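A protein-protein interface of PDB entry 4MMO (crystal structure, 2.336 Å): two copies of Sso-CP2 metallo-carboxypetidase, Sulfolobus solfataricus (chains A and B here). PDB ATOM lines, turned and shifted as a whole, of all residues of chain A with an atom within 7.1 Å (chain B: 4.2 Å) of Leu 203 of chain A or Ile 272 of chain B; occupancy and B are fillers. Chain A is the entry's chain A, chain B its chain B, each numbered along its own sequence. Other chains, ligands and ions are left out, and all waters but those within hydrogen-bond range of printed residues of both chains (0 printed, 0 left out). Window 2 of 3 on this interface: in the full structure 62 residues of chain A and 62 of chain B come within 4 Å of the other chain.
Printed residues of chain B that touch a printed residue of chain A: Leu 255, Leu 264, Lys 265, Tyr 266, Ile 272, Ala 275 and Leu 276. Hydrophobic or aromatic side chains of chain B that line the printed part of chain A: Leu 255, Leu 264, Tyr 266, Ile 272 and Leu 276. Hydrophobic or aromatic side chains of chain A that line the printed part of chain B: Pro 202, Leu 203 and Val 204. Among the printed residues, 10 pairs touch across the chains.
Of the printed residues of chain B, Pro 202 of chain A touches Lys 265 (3.4 Å), Tyr 266 (3.4 Å) and Ala 275 (3.4 Å). Leu 203 of chain A touches four residues of chain B. Of the printed residues of chain A, Leu 255 of chain B touches Leu 203. Printed residues of chain A within 4 Å of Leu 264 of chain B: Leu 203 (3.5 Å) and Val 204 (3.7 Å). Printed residues of chain A within 4 Å of Lys 265 of chain B: Pro 202 (3.4 Å), Leu 203 (2.7 Å) and Val 204 (3.4 Å). Of chain A, only Leu 203 (3.7 Å) comes within 4 Å of Ile 272 of chain B. Ala 273 of chain B touches none of the printed residues of chain A. Printed residues of chain A within 4 Å of Leu 276 of chain B: Ser 199. The nearest residue of chain B that does not touch Leu 203 of chain A is Leu 276 of chain B (4.03 Å). The nearest residue of chain A that does not touch Ile 272 of chain B is Pro 202 of chain A (6.5 Å).
O of Leu 203 of chain A sits at hydrogen-bond distance from N of Lys 265 of chain B.
No position is printed for both chains.
Ser 199 of chain A touches Leu 276 of chain B. Lys 265 of chain B touches Pro 202 of chain A. Tyr 266 of chain B touches Pro 202 of chain A. Pro 202 of chain A touches Ala 275 of chain B (CB to O, 3.4 Å). Leu 255 of chain B touches Leu 203 of chain A. Leu 203 of chain A touches Leu 264 of chain B. CD2 of Leu 203 of chain A touches O of Ile 272 of chain B, at 3.7 Å. Val 204 of chain A touches Leu 264 of chain B. Val 204 of chain A touches Lys 265 of chain B (O to CD, 3.4 Å).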
ATOM      1  N   LEU A 196     -13.588  26.715   0.498  1.00  0.00           N
ATOM      2  CA  LEU A 196     -14.460  26.374   1.611  1.00  0.00           C
ATOM      3  C   LEU A 196     -14.506  24.875   1.802  1.00  0.00           C
ATOM      4  O   LEU A 196     -14.238  24.115   0.874  1.00  0.00           O
ATOM      5  CB  LEU A 196     -15.879  26.865   1.343  1.00  0.00           C
ATOM      6  CG  LEU A 196     -16.012  28.310   0.866  1.00  0.00           C
ATOM      7  CD1 LEU A 196     -17.478  28.648   0.652  1.00  0.00           C
ATOM      8  CD2 LEU A 196     -15.368  29.269   1.848  1.00  0.00           C
ATOM      9  N   SER A 199     -18.618  20.815   2.856  1.00  0.00           N
ATOM     10  CA  SER A 199     -19.831  20.692   3.660  1.00  0.00           C
ATOM     11  C   SER A 199     -20.739  21.917   3.502  1.00  0.00           C
ATOM     12  O   SER A 199     -21.934  21.854   3.791  1.00  0.00           O
ATOM     13  CB  SER A 199     -19.476  20.485   5.133  1.00  0.00           C
ATOM     14  OG  SER A 199     -18.744  21.586   5.635  1.00  0.00           O
ATOM     15  N   ASN A 200     -20.168  23.025   3.033  1.00  0.00           N
ATOM     16  CA  ASN A 200     -20.937  24.241   2.763  1.00  0.00           C
ATOM     17  C   ASN A 200     -21.564  24.279   1.368  1.00  0.00           C
ATOM     18  O   ASN A 200     -22.245  25.244   1.019  1.00  0.00           O
ATOM     19  CB  ASN A 200     -20.047  25.472   2.937  1.00  0.00           C
ATOM     20  CG  ASN A 200     -19.598  25.666   4.366  1.00  0.00           C
ATOM     21  OD1 ASN A 200     -20.355  26.154   5.201  1.00  0.00           O
ATOM     22  ND2 ASN A 200     -18.360  25.288   4.654  1.00  0.00           N
ATOM     23  N   ALA A 201     -21.347  23.226   0.584  1.00  0.00           N
ATOM     24  CA  ALA A 201     -21.764  23.207  -0.825  1.00  0.00           C
ATOM     25  C   ALA A 201     -23.221  23.626  -1.074  1.00  0.00           C
ATOM     26  O   ALA A 201     -23.512  24.266  -2.086  1.00  0.00           O
ATOM     27  CB  ALA A 201     -21.502  21.833  -1.437  1.00  0.00           C
ATOM     28  N   PRO A 202     -24.145  23.263  -0.164  1.00  0.00           N
ATOM     29  CA  PRO A 202     -25.537  23.662  -0.414  1.00  0.00           C
ATOM     30  C   PRO A 202     -25.776  25.175  -0.344  1.00  0.00           C
ATOM     31  O   PRO A 202     -26.801  25.644  -0.841  1.00  0.00           O
ATOM     32  CB  PRO A 202     -26.315  22.956   0.702  1.00  0.00           C
ATOM     33  CG  PRO A 202     -25.434  21.834   1.142  1.00  0.00           C
ATOM     34  CD  PRO A 202     -24.035  22.336   0.977  1.00  0.00           C
ATOM     35  N   LEU A 203     -24.841  25.920   0.244  1.00  0.00           N
ATOM     36  CA  LEU A 203     -25.030  27.352   0.478  1.00  0.00           C
ATOM     37  C   LEU A 203     -24.483  28.248  -0.637  1.00  0.00           C
ATOM     38  O   LEU A 203     -24.838  29.425  -0.718  1.00  0.00           O
ATOM     39  CB  LEU A 203     -24.368  27.761   1.797  1.00  0.00           C
ATOM     40  CG  LEU A 203     -24.793  27.013   3.063  1.00  0.00           C
ATOM     41  CD1 LEU A 203     -24.162  27.670   4.279  1.00  0.00           C
ATOM     42  CD2 LEU A 203     -26.308  26.968   3.200  1.00  0.00           C
ATOM     43  N   VAL A 204     -23.624  27.696  -1.491  1.00  0.00           N
ATOM     44  CA  VAL A 204     -22.919  28.499  -2.487  1.00  0.00           C
ATOM     45  C   VAL A 204     -22.900  27.865  -3.869  1.00  0.00           C
ATOM     46  O   VAL A 204     -23.168  26.673  -4.028  1.00  0.00           O
ATOM     47  CB  VAL A 204     -21.461  28.738  -2.063  1.00  0.00           C
ATOM     48  CG1 VAL A 204     -21.408  29.566  -0.785  1.00  0.00           C
ATOM     49  CG2 VAL A 204     -20.734  27.413  -1.876  1.00  0.00           C
ATOM     50  N   ARG A 205     -22.583  28.683  -4.868  1.00  0.00           N
ATOM     51  CA  ARG A 205     -22.302  28.186  -6.203  1.00  0.00           C
ATOM     52  C   ARG A 205     -20.872  27.667  -6.243  1.00  0.00           C
ATOM     53  O   ARG A 205     -19.991  28.189  -5.560  1.00  0.00           O
ATOM     54  CB  ARG A 205     -22.478  29.294  -7.240  1.00  0.00           C
ATOM     55  CG  ARG A 205     -23.892  29.840  -7.342  1.00  0.00           C
ATOM     56  CD  ARG A 205     -24.113  30.529  -8.677  1.00  0.00           C
ATOM     57  NE  ARG A 205     -24.065  29.579  -9.787  1.00  0.00           N
ATOM     58  CZ  ARG A 205     -25.115  28.903 -10.246  1.00  0.00           C
ATOM     59  NH1 ARG A 205     -26.314  29.066  -9.705  1.00  0.00           N
ATOM     60  NH2 ARG A 205     -24.966  28.059 -11.256  1.00  0.00           N
ATOM     61  N   VAL B 252     -26.623  35.140   9.886  1.00  0.00           N
ATOM     62  CA  VAL B 252     -26.344  35.110   8.454  1.00  0.00           C
ATOM     63  C   VAL B 252     -25.147  35.982   8.087  1.00  0.00           C
ATOM     64  O   VAL B 252     -24.253  35.544   7.359  1.00  0.00           O
ATOM     65  CB  VAL B 252     -27.576  35.571   7.639  1.00  0.00           C
ATOM     66  CG1 VAL B 252     -27.272  35.595   6.139  1.00  0.00           C
ATOM     67  CG2 VAL B 252     -28.765  34.666   7.923  1.00  0.00           C
ATOM     68  N   LEU B 255     -21.970  34.388   9.168  1.00  0.00           N
ATOM     69  CA  LEU B 255     -21.667  33.206   8.370  1.00  0.00           C
ATOM     70  C   LEU B 255     -21.104  33.630   7.022  1.00  0.00           C
ATOM     71  O   LEU B 255     -20.064  33.136   6.591  1.00  0.00           O
ATOM     72  CB  LEU B 255     -22.921  32.352   8.161  1.00  0.00           C
ATOM     73  CG  LEU B 255     -22.752  31.142   7.235  1.00  0.00           C
ATOM     74  CD1 LEU B 255     -21.750  30.144   7.805  1.00  0.00           C
ATOM     75  CD2 LEU B 255     -24.093  30.470   6.977  1.00  0.00           C
ATOM     76  N   LEU B 264     -24.183  34.180  -1.169  1.00  0.00           N
ATOM     77  CA  LEU B 264     -24.745  32.894  -0.784  1.00  0.00           C
ATOM     78  C   LEU B 264     -26.030  32.667  -1.569  1.00  0.00           C
ATOM     79  O   LEU B 264     -26.683  33.623  -1.986  1.00  0.00           O
ATOM     80  CB  LEU B 264     -25.047  32.866   0.714  1.00  0.00           C
ATOM     81  CG  LEU B 264     -23.880  33.124   1.669  1.00  0.00           C
ATOM     82  CD1 LEU B 264     -24.345  32.955   3.105  1.00  0.00           C
ATOM     83  CD2 LEU B 264     -22.705  32.206   1.378  1.00  0.00           C
ATOM     84  N   LYS B 265     -26.392  31.404  -1.766  1.00  0.00           N
ATOM     85  CA  LYS B 265     -27.594  31.070  -2.524  1.00  0.00           C
ATOM     86  C   LYS B 265     -28.855  31.484  -1.774  1.00  0.00           C
ATOM     87  O   LYS B 265     -29.893  31.734  -2.386  1.00  0.00           O
ATOM     88  CB  LYS B 265     -27.642  29.570  -2.818  1.00  0.00           C
ATOM     89  CG  LYS B 265     -26.517  29.068  -3.710  1.00  0.00           C
ATOM     90  CD  LYS B 265     -26.426  27.547  -3.684  1.00  0.00           C
ATOM     91  CE  LYS B 265     -27.559  26.892  -4.452  1.00  0.00           C
ATOM     92  NZ  LYS B 265     -27.333  26.950  -5.924  1.00  0.00           N
ATOM     93  N   TYR B 266     -28.759  31.552  -0.448  1.00  0.00           N
ATOM     94  CA  TYR B 266     -29.893  31.930   0.390  1.00  0.00           C
ATOM     95  C   TYR B 266     -29.501  33.007   1.401  1.00  0.00           C
ATOM     96  O   TYR B 266     -28.350  33.068   1.839  1.00  0.00           O
ATOM     97  CB  TYR B 266     -30.431  30.707   1.134  1.00  0.00           C
ATOM     98  CG  TYR B 266     -30.543  29.462   0.284  1.00  0.00           C
ATOM     99  CD1 TYR B 266     -31.574  29.312  -0.634  1.00  0.00           C
ATOM    100  CD2 TYR B 266     -29.622  28.431   0.407  1.00  0.00           C
ATOM    101  CE1 TYR B 266     -31.681  28.174  -1.406  1.00  0.00           C
ATOM    102  CE2 TYR B 266     -29.721  27.288  -0.361  1.00  0.00           C
ATOM    103  CZ  TYR B 266     -30.753  27.165  -1.265  1.00  0.00           C
ATOM    104  OH  TYR B 266     -30.854  26.028  -2.031  1.00  0.00           O
ATOM    105  N   GLU B 268     -32.098  33.969   4.007  1.00  0.00           N
ATOM    106  CA  GLU B 268     -32.898  33.691   5.198  1.00  0.00           C
ATOM    107  C   GLU B 268     -32.256  32.590   6.040  1.00  0.00           C
ATOM    108  O   GLU B 268     -31.814  31.572   5.507  1.00  0.00           O
ATOM    109  CB  GLU B 268     -34.313  33.282   4.789  1.00  0.00           C
ATOM    110  CG  GLU B 268     -35.037  34.336   3.955  1.00  0.00           C
ATOM    111  CD  GLU B 268     -36.266  33.795   3.246  1.00  0.00           C
ATOM    112  OE1 GLU B 268     -36.294  32.589   2.919  1.00  0.00           O
ATOM    113  OE2 GLU B 268     -37.209  34.581   3.012  1.00  0.00           O
ATOM    114  N   LYS B 269     -32.213  32.797   7.354  1.00  0.00           N
ATOM    115  CA  LYS B 269     -31.534  31.873   8.262  1.00  0.00           C
ATOM    116  C   LYS B 269     -32.188  30.492   8.293  1.00  0.00           C
ATOM    117  O   LYS B 269     -31.501  29.478   8.400  1.00  0.00           O
ATOM    118  CB  LYS B 269     -31.471  32.456   9.676  1.00  0.00           C
ATOM    119  CG  LYS B 269     -32.821  32.846  10.261  1.00  0.00           C
ATOM    120  CD  LYS B 269     -32.705  33.288  11.717  1.00  0.00           C
ATOM    121  CE  LYS B 269     -31.747  34.460  11.884  1.00  0.00           C
ATOM    122  NZ  LYS B 269     -31.787  35.027  13.261  1.00  0.00           N
ATOM    123  N   GLU B 270     -33.513  30.459   8.206  1.00  0.00           N
ATOM    124  CA  GLU B 270     -34.248  29.202   8.142  1.00  0.00           C
ATOM    125  C   GLU B 270     -33.793  28.407   6.922  1.00  0.00           C
ATOM    126  O   GLU B 270     -33.463  27.224   7.021  1.00  0.00           O
ATOM    127  CB  GLU B 270     -35.753  29.481   8.059  1.00  0.00           C
ATOM    128  CG  GLU B 270     -36.642  28.264   7.787  1.00  0.00           C
ATOM    129  CD  GLU B 270     -36.815  27.371   9.001  1.00  0.00           C
ATOM    130  OE1 GLU B 270     -35.975  27.440   9.921  1.00  0.00           O
ATOM    131  OE2 GLU B 270     -37.801  26.604   9.037  1.00  0.00           O
ATOM    132  N   LYS B 271     -33.780  29.075   5.774  1.00  0.00           N
ATOM    133  CA  LYS B 271     -33.401  28.446   4.519  1.00  0.00           C
ATOM    134  C   LYS B 271     -31.970  27.911   4.583  1.00  0.00           C
ATOM    135  O   LYS B 271     -31.691  26.802   4.126  1.00  0.00           O
ATOM    136  CB  LYS B 271     -33.532  29.452   3.376  1.00  0.00           C
ATOM    137  CG  LYS B 271     -33.551  28.826   1.995  1.00  0.00           C
ATOM    138  CD  LYS B 271     -34.916  28.237   1.670  1.00  0.00           C
ATOM    139  CE  LYS B 271     -34.821  27.145   0.615  1.00  0.00           C
ATOM    140  NZ  LYS B 271     -36.161  26.592   0.270  1.00  0.00           N
ATOM    141  N   ILE B 272     -31.067  28.701   5.158  1.00  0.00           N
ATOM    142  CA  ILE B 272     -29.666  28.310   5.258  1.00  0.00           C
ATOM    143  C   ILE B 272     -29.508  27.066   6.128  1.00  0.00           C
ATOM    144  O   ILE B 272     -28.765  26.149   5.779  1.00  0.00           O
ATOM    145  CB  ILE B 272     -28.797  29.466   5.812  1.00  0.00           C
ATOM    146  CG1 ILE B 272     -28.545  30.492   4.705  1.00  0.00           C
ATOM    147  CG2 ILE B 272     -27.460  28.948   6.364  1.00  0.00           C
ATOM    148  CD1 ILE B 272     -27.789  31.730   5.147  1.00  0.00           C
ATOM    149  N   ALA B 273     -30.201  27.045   7.261  1.00  0.00           N
ATOM    150  CA  ALA B 273     -30.127  25.916   8.175  1.00  0.00           C
ATOM    151  C   ALA B 273     -30.624  24.656   7.479  1.00  0.00           C
ATOM    152  O   ALA B 273     -30.014  23.591   7.575  1.00  0.00           O
ATOM    153  CB  ALA B 273     -30.953  26.192   9.419  1.00  0.00           C
ATOM    154  N   GLU B 274     -31.733  24.795   6.764  1.00  0.00           N
ATOM    155  CA  GLU B 274     -32.345  23.668   6.082  1.00  0.00           C
ATOM    156  C   GLU B 274     -31.404  23.098   5.023  1.00  0.00           C
ATOM    157  O   GLU B 274     -31.162  21.896   4.986  1.00  0.00           O
ATOM    158  CB  GLU B 274     -33.670  24.096   5.454  1.00  0.00           C
ATOM    159  CG  GLU B 274     -34.580  22.943   5.075  1.00  0.00           C
ATOM    160  CD  GLU B 274     -35.967  23.406   4.679  1.00  0.00           C
ATOM    161  OE1 GLU B 274     -36.517  24.296   5.365  1.00  0.00           O
ATOM    162  OE2 GLU B 274     -36.508  22.883   3.683  1.00  0.00           O
ATOM    163  N   ALA B 275     -30.852  23.963   4.179  1.00  0.00           N
ATOM    164  CA  ALA B 275     -29.982  23.511   3.099  1.00  0.00           C
ATOM    165  C   ALA B 275     -28.694  22.891   3.633  1.00  0.00           C
ATOM    166  O   ALA B 275     -28.270  21.822   3.190  1.00  0.00           O
ATOM    167  CB  ALA B 275     -29.661  24.664   2.158  1.00  0.00           C
ATOM    168  N   LEU B 276     -28.076  23.568   4.592  1.00  0.00           N
ATOM    169  CA  LEU B 276     -26.788  23.148   5.125  1.00  0.00           C
ATOM    170  C   LEU B 276     -26.848  21.771   5.790  1.00  0.00           C
ATOM    171  O   LEU B 276     -25.887  21.002   5.719  1.00  0.00           O
ATOM    172  CB  LEU B 276     -26.283  24.191   6.127  1.00  0.00           C
ATOM    173  CG  LEU B 276     -24.949  23.905   6.817  1.00  0.00           C
ATOM    174  CD1 LEU B 276     -23.821  23.789   5.800  1.00  0.00           C
ATOM    175  CD2 LEU B 276     -24.644  24.990   7.842  1.00  0.00           C
